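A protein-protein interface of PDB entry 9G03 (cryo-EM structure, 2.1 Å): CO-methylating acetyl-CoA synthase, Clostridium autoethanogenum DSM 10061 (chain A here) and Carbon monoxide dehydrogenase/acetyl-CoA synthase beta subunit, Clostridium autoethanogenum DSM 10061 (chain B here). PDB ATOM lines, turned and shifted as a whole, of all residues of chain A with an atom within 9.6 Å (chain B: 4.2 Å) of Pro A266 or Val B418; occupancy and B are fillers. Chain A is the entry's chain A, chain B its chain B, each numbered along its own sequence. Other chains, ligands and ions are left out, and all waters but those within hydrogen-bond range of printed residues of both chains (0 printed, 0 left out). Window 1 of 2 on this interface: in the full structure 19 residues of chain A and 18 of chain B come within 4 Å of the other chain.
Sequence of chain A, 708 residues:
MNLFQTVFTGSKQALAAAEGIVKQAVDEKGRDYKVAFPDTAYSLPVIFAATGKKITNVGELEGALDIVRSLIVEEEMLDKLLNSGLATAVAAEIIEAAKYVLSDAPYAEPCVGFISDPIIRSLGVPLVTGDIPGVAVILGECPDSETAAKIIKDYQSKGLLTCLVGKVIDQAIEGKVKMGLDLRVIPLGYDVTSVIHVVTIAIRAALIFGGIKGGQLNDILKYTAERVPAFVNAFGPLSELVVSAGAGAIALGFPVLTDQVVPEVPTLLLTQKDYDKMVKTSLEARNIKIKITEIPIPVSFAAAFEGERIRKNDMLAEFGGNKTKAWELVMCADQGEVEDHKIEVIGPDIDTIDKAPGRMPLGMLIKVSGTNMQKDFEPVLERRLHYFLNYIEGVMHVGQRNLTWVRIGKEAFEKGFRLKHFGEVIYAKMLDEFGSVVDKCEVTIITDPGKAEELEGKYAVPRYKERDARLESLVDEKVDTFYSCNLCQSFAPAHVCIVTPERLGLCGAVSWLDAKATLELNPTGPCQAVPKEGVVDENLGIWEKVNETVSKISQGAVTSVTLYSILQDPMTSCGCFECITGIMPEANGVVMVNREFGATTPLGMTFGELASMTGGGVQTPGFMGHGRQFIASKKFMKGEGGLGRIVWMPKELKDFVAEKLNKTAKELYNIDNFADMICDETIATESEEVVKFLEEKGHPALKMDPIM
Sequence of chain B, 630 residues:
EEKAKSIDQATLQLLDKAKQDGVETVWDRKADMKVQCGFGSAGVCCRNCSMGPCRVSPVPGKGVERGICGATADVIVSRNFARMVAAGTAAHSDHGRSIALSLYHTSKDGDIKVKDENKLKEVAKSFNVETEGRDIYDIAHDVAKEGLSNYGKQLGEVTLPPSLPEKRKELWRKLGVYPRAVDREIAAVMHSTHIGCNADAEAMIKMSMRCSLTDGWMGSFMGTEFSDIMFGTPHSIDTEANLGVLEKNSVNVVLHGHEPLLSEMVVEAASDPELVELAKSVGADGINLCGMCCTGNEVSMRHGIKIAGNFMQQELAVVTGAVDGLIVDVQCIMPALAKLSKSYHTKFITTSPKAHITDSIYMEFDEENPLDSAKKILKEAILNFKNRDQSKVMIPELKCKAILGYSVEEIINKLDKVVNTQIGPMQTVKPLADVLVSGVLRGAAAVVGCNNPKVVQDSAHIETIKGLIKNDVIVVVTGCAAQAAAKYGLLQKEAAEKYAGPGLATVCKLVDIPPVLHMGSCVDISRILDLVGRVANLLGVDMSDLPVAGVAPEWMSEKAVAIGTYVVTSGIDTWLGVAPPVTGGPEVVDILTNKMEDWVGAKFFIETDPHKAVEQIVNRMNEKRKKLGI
Val B418 touches Pro A266 (O to CB, 3.6 Å).
Pro A266 touches Val B435.
Leu B510 touches Pro A266.
Val B418 touches Thr A267 (CB to CG2, 3.95 Å).
Leu B510 touches Thr A267 (CD1 to OG1, 3.5 Å).
Leu A270 touches Asn B420 (CD1 to ND2, 3.9 Å).
Asn B420 touches Ala A285.
Hydrophobic or aromatic side chains of chain A that line the printed part of chain B: Pro A266, Leu A270 and Ala A285.
Along chain A the printed residues that touch a printed residue of chain B span positions 266 to 285.
Hydrophobic or aromatic side chains of chain B that line the printed part of chain A: Val B418, Val B435 and Leu B510.
Among the printed residues, no Asp or Glu carboxylate lies within 4 Å of a Lys or Arg side-chain nitrogen of the other chain.
OE1 of Glu A284 lies close to OD1 of Asn B420, 3.2 Å away.
The backbone carbonyl oxygen (O) of Val A256 is in hydrogen-bond range of the backbone NH (N) of Leu A270 (3.0 Å).
Pro A266 touches just these residues of chain B: Val B418, Val B435 and Leu B510.
Of the printed residues of chain B, Thr A267 touches Val B418 and Leu B510.
Leu A269 touches none of the printed residues of chain B.
Printed residues of chain B within 4 Å of Leu A270: Asn B420.
Of the printed residues of chain B, Glu A284 touches Asn B420 (3.2 Å).
Val B418 touches two residues of chain A.
No residue of chain A comes within 4 Å of Val B419.
Of the printed residues of chain A, Asn B420 touches Leu A270, Glu A284 and Ala A285.
The nearest residue of chain A that does not touch Val B418 is Leu A270 (5.7 Å).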
ATOM      1  N   LEU A   3     -29.680 -23.979 -19.747  1.00  0.00           N
ATOM      2  CA  LEU A   3     -30.210 -23.878 -18.390  1.00  0.00           C
ATOM      3  C   LEU A   3     -31.407 -22.936 -18.313  1.00  0.00           C
ATOM      4  O   LEU A   3     -32.430 -23.266 -17.704  1.00  0.00           O
ATOM      5  CB  LEU A   3     -29.111 -23.411 -17.434  1.00  0.00           C
ATOM      6  CG  LEU A   3     -29.523 -23.269 -15.964  1.00  0.00           C
ATOM      7  CD1 LEU A   3     -29.949 -24.600 -15.367  1.00  0.00           C
ATOM      8  CD2 LEU A   3     -28.392 -22.652 -15.153  1.00  0.00           C
ATOM      9  N   LEU A  78     -29.813 -13.565 -15.338  1.00  0.00           N
ATOM     10  CA  LEU A  78     -29.881 -14.319 -14.089  1.00  0.00           C
ATOM     11  C   LEU A  78     -31.107 -13.940 -13.258  1.00  0.00           C
ATOM     12  O   LEU A  78     -31.737 -14.806 -12.639  1.00  0.00           O
ATOM     13  CB  LEU A  78     -28.604 -14.111 -13.287  1.00  0.00           C
ATOM     14  CG  LEU A  78     -28.535 -14.871 -11.962  1.00  0.00           C
ATOM     15  CD1 LEU A  78     -28.583 -16.372 -12.175  1.00  0.00           C
ATOM     16  CD2 LEU A  78     -27.280 -14.477 -11.213  1.00  0.00           C
ATOM     17  N   ILE A 250     -32.513 -22.072  -5.536  1.00  0.00           N
ATOM     18  CA  ILE A 250     -31.388 -21.159  -5.717  1.00  0.00           C
ATOM     19  C   ILE A 250     -31.817 -19.719  -5.464  1.00  0.00           C
ATOM     20  O   ILE A 250     -31.091 -18.947  -4.830  1.00  0.00           O
ATOM     21  CB  ILE A 250     -30.772 -21.341  -7.120  1.00  0.00           C
ATOM     22  CG1 ILE A 250     -30.177 -22.751  -7.252  1.00  0.00           C
ATOM     23  CG2 ILE A 250     -29.708 -20.289  -7.384  1.00  0.00           C
ATOM     24  CD1 ILE A 250     -29.649 -23.091  -8.612  1.00  0.00           C
ATOM     25  N   PRO A 255     -28.220 -23.849  -2.258  1.00  0.00           N
ATOM     26  CA  PRO A 255     -27.529 -24.526  -3.361  1.00  0.00           C
ATOM     27  C   PRO A 255     -28.139 -25.876  -3.705  1.00  0.00           C
ATOM     28  O   PRO A 255     -28.683 -26.581  -2.857  1.00  0.00           O
ATOM     29  CB  PRO A 255     -26.096 -24.685  -2.838  1.00  0.00           C
ATOM     30  CG  PRO A 255     -26.215 -24.639  -1.361  1.00  0.00           C
ATOM     31  CD  PRO A 255     -27.386 -23.777  -1.042  1.00  0.00           C
ATOM     32  N   VAL A 256     -28.078 -26.217  -4.982  1.00  0.00           N
ATOM     33  CA  VAL A 256     -28.659 -27.452  -5.482  1.00  0.00           C
ATOM     34  C   VAL A 256     -27.519 -28.354  -5.946  1.00  0.00           C
ATOM     35  O   VAL A 256     -26.700 -27.960  -6.782  1.00  0.00           O
ATOM     36  CB  VAL A 256     -29.671 -27.188  -6.607  1.00  0.00           C
ATOM     37  CG1 VAL A 256     -30.175 -28.500  -7.201  1.00  0.00           C
ATOM     38  CG2 VAL A 256     -30.832 -26.338  -6.083  1.00  0.00           C
ATOM     39  N   VAL A 262     -25.477 -31.447 -15.358  1.00  0.00           N
ATOM     40  CA  VAL A 262     -26.252 -30.221 -15.529  1.00  0.00           C
ATOM     41  C   VAL A 262     -25.286 -29.086 -15.837  1.00  0.00           C
ATOM     42  O   VAL A 262     -24.079 -29.197 -15.577  1.00  0.00           O
ATOM     43  CB  VAL A 262     -27.101 -29.900 -14.277  1.00  0.00           C
ATOM     44  CG1 VAL A 262     -28.110 -31.002 -14.020  1.00  0.00           C
ATOM     45  CG2 VAL A 262     -26.206 -29.695 -13.062  1.00  0.00           C
ATOM     46  N   PRO A 263     -25.778 -27.981 -16.406  1.00  0.00           N
ATOM     47  CA  PRO A 263     -24.905 -26.810 -16.562  1.00  0.00           C
ATOM     48  C   PRO A 263     -24.593 -26.202 -15.205  1.00  0.00           C
ATOM     49  O   PRO A 263     -25.422 -25.509 -14.608  1.00  0.00           O
ATOM     50  CB  PRO A 263     -25.731 -25.859 -17.439  1.00  0.00           C
ATOM     51  CG  PRO A 263     -26.744 -26.717 -18.086  1.00  0.00           C
ATOM     52  CD  PRO A 263     -27.055 -27.801 -17.111  1.00  0.00           C
ATOM     53  N   GLU A 264     -23.377 -26.432 -14.729  1.00  0.00           N
ATOM     54  CA  GLU A 264     -23.020 -26.081 -13.365  1.00  0.00           C
ATOM     55  C   GLU A 264     -22.892 -24.574 -13.192  1.00  0.00           C
ATOM     56  O   GLU A 264     -22.453 -23.859 -14.093  1.00  0.00           O
ATOM     57  CB  GLU A 264     -21.715 -26.770 -12.970  1.00  0.00           C
ATOM     58  CG  GLU A 264     -21.904 -28.221 -12.536  1.00  0.00           C
ATOM     59  CD  GLU A 264     -20.605 -28.910 -12.166  1.00  0.00           C
ATOM     60  OE1 GLU A 264     -19.701 -28.986 -13.024  1.00  0.00           O
ATOM     61  OE2 GLU A 264     -20.487 -29.382 -11.018  1.00  0.00           O
ATOM     62  N   VAL A 265     -23.301 -24.101 -12.024  1.00  0.00           N
ATOM     63  CA  VAL A 265     -23.112 -22.725 -11.593  1.00  0.00           C
ATOM     64  C   VAL A 265     -22.344 -22.788 -10.275  1.00  0.00           C
ATOM     65  O   VAL A 265     -22.840 -23.365  -9.303  1.00  0.00           O
ATOM     66  CB  VAL A 265     -24.445 -21.974 -11.425  1.00  0.00           C
ATOM     67  CG1 VAL A 265     -24.203 -20.552 -10.955  1.00  0.00           C
ATOM     68  CG2 VAL A 265     -25.236 -21.984 -12.741  1.00  0.00           C
ATOM     69  N   PRO A 266     -21.147 -22.207 -10.184  1.00  0.00           N
ATOM     70  CA  PRO A 266     -20.350 -22.345  -8.958  1.00  0.00           C
ATOM     71  C   PRO A 266     -21.101 -21.883  -7.721  1.00  0.00           C
ATOM     72  O   PRO A 266     -21.726 -20.823  -7.703  1.00  0.00           O
ATOM     73  CB  PRO A 266     -19.126 -21.467  -9.232  1.00  0.00           C
ATOM     74  CG  PRO A 266     -19.002 -21.466 -10.705  1.00  0.00           C
ATOM     75  CD  PRO A 266     -20.395 -21.509 -11.240  1.00  0.00           C
ATOM     76  N   THR A 267     -20.989 -22.692  -6.672  1.00  0.00           N
ATOM     77  CA  THR A 267     -21.593 -22.463  -5.362  1.00  0.00           C
ATOM     78  C   THR A 267     -23.118 -22.561  -5.380  1.00  0.00           C
ATOM     79  O   THR A 267     -23.736 -22.551  -4.313  1.00  0.00           O
ATOM     80  CB  THR A 267     -21.211 -21.077  -4.799  1.00  0.00           C
ATOM     81  OG1 THR A 267     -21.948 -20.047  -5.468  1.00  0.00           O
ATOM     82  CG2 THR A 267     -19.713 -20.791  -4.926  1.00  0.00           C
ATOM     83  N   LEU A 268     -23.735 -22.729  -6.550  1.00  0.00           N
ATOM     84  CA  LEU A 268     -25.192 -22.745  -6.648  1.00  0.00           C
ATOM     85  C   LEU A 268     -25.724 -24.042  -7.233  1.00  0.00           C
ATOM     86  O   LEU A 268     -26.631 -24.644  -6.659  1.00  0.00           O
ATOM     87  CB  LEU A 268     -25.690 -21.551  -7.478  1.00  0.00           C
ATOM     88  CG  LEU A 268     -25.379 -20.164  -6.902  1.00  0.00           C
ATOM     89  CD1 LEU A 268     -25.965 -19.073  -7.775  1.00  0.00           C
ATOM     90  CD2 LEU A 268     -25.896 -20.031  -5.485  1.00  0.00           C
ATOM     91  N   LEU A 269     -25.183 -24.497  -8.355  1.00  0.00           N
ATOM     92  CA  LEU A 269     -25.643 -25.717  -9.007  1.00  0.00           C
ATOM     93  C   LEU A 269     -24.416 -26.575  -9.263  1.00  0.00           C
ATOM     94  O   LEU A 269     -23.539 -26.200 -10.047  1.00  0.00           O
ATOM     95  CB  LEU A 269     -26.399 -25.402 -10.294  1.00  0.00           C
ATOM     96  CG  LEU A 269     -27.036 -26.592 -11.006  1.00  0.00           C
ATOM     97  CD1 LEU A 269     -27.991 -27.323 -10.104  1.00  0.00           C
ATOM     98  CD2 LEU A 269     -27.745 -26.118 -12.262  1.00  0.00           C
ATOM     99  N   LEU A 270     -24.346 -27.714  -8.588  1.00  0.00           N
ATOM    100  CA  LEU A 270     -23.152 -28.541  -8.573  1.00  0.00           C
ATOM    101  C   LEU A 270     -23.489 -29.992  -8.876  1.00  0.00           C
ATOM    102  O   LEU A 270     -24.505 -30.517  -8.414  1.00  0.00           O
ATOM    103  CB  LEU A 270     -22.445 -28.443  -7.215  1.00  0.00           C
ATOM    104  CG  LEU A 270     -22.074 -27.046  -6.705  1.00  0.00           C
ATOM    105  CD1 LEU A 270     -21.433 -27.152  -5.334  1.00  0.00           C
ATOM    106  CD2 LEU A 270     -21.153 -26.322  -7.665  1.00  0.00           C
ATOM    107  N   THR A 271     -22.616 -30.636  -9.638  1.00  0.00           N
ATOM    108  CA  THR A 271     -22.750 -32.048  -9.956  1.00  0.00           C
ATOM    109  C   THR A 271     -21.747 -32.847  -9.138  1.00  0.00           C
ATOM    110  O   THR A 271     -20.555 -32.532  -9.134  1.00  0.00           O
ATOM    111  CB  THR A 271     -22.523 -32.301 -11.453  1.00  0.00           C
ATOM    112  OG1 THR A 271     -23.586 -31.719 -12.212  1.00  0.00           O
ATOM    113  CG2 THR A 271     -22.450 -33.785 -11.757  1.00  0.00           C
ATOM    114  N   GLU A 284     -20.008 -28.638   2.629  1.00  0.00           N
ATOM    115  CA  GLU A 284     -19.113 -27.577   2.177  1.00  0.00           C
ATOM    116  C   GLU A 284     -19.858 -26.526   1.366  1.00  0.00           C
ATOM    117  O   GLU A 284     -19.608 -25.329   1.518  1.00  0.00           O
ATOM    118  CB  GLU A 284     -17.956 -28.155   1.360  1.00  0.00           C
ATOM    119  CG  GLU A 284     -17.015 -27.089   0.836  1.00  0.00           C
ATOM    120  CD  GLU A 284     -15.919 -27.643  -0.034  1.00  0.00           C
ATOM    121  OE1 GLU A 284     -15.732 -28.873  -0.049  1.00  0.00           O
ATOM    122  OE2 GLU A 284     -15.250 -26.846  -0.719  1.00  0.00           O
ATOM    123  N   ALA A 285     -20.770 -26.954   0.492  1.00  0.00           N
ATOM    124  CA  ALA A 285     -21.462 -26.003  -0.368  1.00  0.00           C
ATOM    125  C   ALA A 285     -22.373 -25.094   0.438  1.00  0.00           C
ATOM    126  O   ALA A 285     -22.529 -23.917   0.100  1.00  0.00           O
ATOM    127  CB  ALA A 285     -22.256 -26.742  -1.443  1.00  0.00           C
ATOM    128  N   LEU B 415     -10.477 -17.815  -9.169  1.00  0.00           N
ATOM    129  CA  LEU B 415     -11.541 -18.759  -9.487  1.00  0.00           C
ATOM    130  C   LEU B 415     -11.518 -19.977  -8.574  1.00  0.00           C
ATOM    131  O   LEU B 415     -12.557 -20.602  -8.350  1.00  0.00           O
ATOM    132  CB  LEU B 415     -11.422 -19.192 -10.945  1.00  0.00           C
ATOM    133  CG  LEU B 415     -11.695 -18.124 -12.006  1.00  0.00           C
ATOM    134  CD1 LEU B 415     -11.369 -18.683 -13.376  1.00  0.00           C
ATOM    135  CD2 LEU B 415     -13.135 -17.647 -11.953  1.00  0.00           C
ATOM    136  N   ASP B 416     -10.356 -20.310  -8.018  1.00  0.00           N
ATOM    137  CA  ASP B 416     -10.286 -21.424  -7.081  1.00  0.00           C
ATOM    138  C   ASP B 416     -11.184 -21.217  -5.865  1.00  0.00           C
ATOM    139  O   ASP B 416     -11.566 -22.195  -5.221  1.00  0.00           O
ATOM    140  CB  ASP B 416      -8.842 -21.637  -6.606  1.00  0.00           C
ATOM    141  CG  ASP B 416      -8.011 -22.461  -7.579  1.00  0.00           C
ATOM    142  OD1 ASP B 416      -8.504 -22.795  -8.678  1.00  0.00           O
ATOM    143  OD2 ASP B 416      -6.855 -22.780  -7.239  1.00  0.00           O
ATOM    144  N   LYS B 417     -11.547 -19.970  -5.557  1.00  0.00           N
ATOM    145  CA  LYS B 417     -12.386 -19.688  -4.394  1.00  0.00           C
ATOM    146  C   LYS B 417     -13.764 -20.329  -4.523  1.00  0.00           C
ATOM    147  O   LYS B 417     -14.323 -20.805  -3.532  1.00  0.00           O
ATOM    148  CB  LYS B 417     -12.511 -18.172  -4.211  1.00  0.00           C
ATOM    149  CG  LYS B 417     -13.551 -17.716  -3.193  1.00  0.00           C
ATOM    150  CD  LYS B 417     -13.751 -16.211  -3.245  1.00  0.00           C
ATOM    151  CE  LYS B 417     -13.377 -15.543  -1.934  1.00  0.00           C
ATOM    152  NZ  LYS B 417     -14.291 -15.933  -0.827  1.00  0.00           N
ATOM    153  N   VAL B 418     -14.321 -20.354  -5.727  1.00  0.00           N
ATOM    154  CA  VAL B 418     -15.677 -20.846  -5.953  1.00  0.00           C
ATOM    155  C   VAL B 418     -15.687 -22.320  -6.372  1.00  0.00           C
ATOM    156  O   VAL B 418     -16.678 -22.792  -6.920  1.00  0.00           O
ATOM    157  CB  VAL B 418     -16.433 -19.976  -6.975  1.00  0.00           C
ATOM    158  CG1 VAL B 418     -16.588 -18.550  -6.461  1.00  0.00           C
ATOM    159  CG2 VAL B 418     -15.745 -19.998  -8.327  1.00  0.00           C
ATOM    160  N   VAL B 419     -14.598 -23.049  -6.140  1.00  0.00           N
ATOM    161  CA  VAL B 419     -14.517 -24.470  -6.465  1.00  0.00           C
ATOM    162  C   VAL B 419     -14.827 -25.262  -5.198  1.00  0.00           C
ATOM    163  O   VAL B 419     -14.145 -25.104  -4.179  1.00  0.00           O
ATOM    164  CB  VAL B 419     -13.124 -24.845  -7.005  1.00  0.00           C
ATOM    165  CG1 VAL B 419     -13.011 -26.354  -7.211  1.00  0.00           C
ATOM    166  CG2 VAL B 419     -12.813 -24.107  -8.293  1.00  0.00           C
ATOM    167  N   ASN B 420     -15.831 -26.137  -5.265  1.00  0.00           N
ATOM    168  CA  ASN B 420     -16.103 -27.041  -4.152  1.00  0.00           C
ATOM    169  C   ASN B 420     -14.945 -28.024  -4.012  1.00  0.00           C
ATOM    170  O   ASN B 420     -14.603 -28.728  -4.963  1.00  0.00           O
ATOM    171  CB  ASN B 420     -17.431 -27.778  -4.368  1.00  0.00           C
ATOM    172  CG  ASN B 420     -17.925 -28.513  -3.111  1.00  0.00           C
ATOM    173  OD1 ASN B 420     -17.384 -29.542  -2.727  1.00  0.00           O
ATOM    174  ND2 ASN B 420     -18.974 -27.991  -2.491  1.00  0.00           N
ATOM    175  N   PRO B 431     -14.299 -22.899 -13.447  1.00  0.00           N
ATOM    176  CA  PRO B 431     -15.412 -22.045 -12.986  1.00  0.00           C
ATOM    177  C   PRO B 431     -15.837 -20.995 -14.009  1.00  0.00           C
ATOM    178  O   PRO B 431     -17.040 -20.729 -14.161  1.00  0.00           O
ATOM    179  CB  PRO B 431     -14.859 -21.418 -11.698  1.00  0.00           C
ATOM    180  CG  PRO B 431     -13.834 -22.378 -11.222  1.00  0.00           C
ATOM    181  CD  PRO B 431     -13.215 -22.967 -12.454  1.00  0.00           C
ATOM    182  N   VAL B 435     -19.565 -20.705 -15.695  1.00  0.00           N
ATOM    183  CA  VAL B 435     -20.445 -19.535 -15.684  1.00  0.00           C
ATOM    184  C   VAL B 435     -20.780 -19.107 -17.110  1.00  0.00           C
ATOM    185  O   VAL B 435     -21.909 -18.682 -17.383  1.00  0.00           O
ATOM    186  CB  VAL B 435     -19.858 -18.363 -14.864  1.00  0.00           C
ATOM    187  CG1 VAL B 435     -19.647 -18.784 -13.422  1.00  0.00           C
ATOM    188  CG2 VAL B 435     -18.573 -17.835 -15.475  1.00  0.00           C
ATOM    189  N   LEU B 510     -19.151 -13.383  -5.817  1.00  0.00           N
ATOM    190  CA  LEU B 510     -18.689 -14.723  -5.459  1.00  0.00           C
ATOM    191  C   LEU B 510     -17.176 -14.847  -5.570  1.00  0.00           C
ATOM    192  O   LEU B 510     -16.535 -15.430  -4.693  1.00  0.00           O
ATOM    193  CB  LEU B 510     -19.372 -15.769  -6.339  1.00  0.00           C
ATOM    194  CG  LEU B 510     -20.868 -15.991  -6.100  1.00  0.00           C
ATOM    195  CD1 LEU B 510     -21.424 -16.967  -7.114  1.00  0.00           C
ATOM    196  CD2 LEU B 510     -21.130 -16.484  -4.691  1.00  0.00           C
ATOM    197  N   VAL B 511     -16.588 -14.313  -6.640  1.00  0.00           N
ATOM    198  CA  VAL B 511     -15.152 -14.441  -6.870  1.00  0.00           C
ATOM    199  C   VAL B 511     -14.366 -13.304  -6.227  1.00  0.00           C
ATOM    200  O   VAL B 511     -13.134 -13.403  -6.118  1.00  0.00           O
ATOM    201  CB  VAL B 511     -14.857 -14.527  -8.384  1.00  0.00           C
ATOM    202  CG1 VAL B 511     -13.394 -14.912  -8.648  1.00  0.00           C
ATOM    203  CG2 VAL B 511     -15.792 -15.528  -9.052  1.00  0.00           C
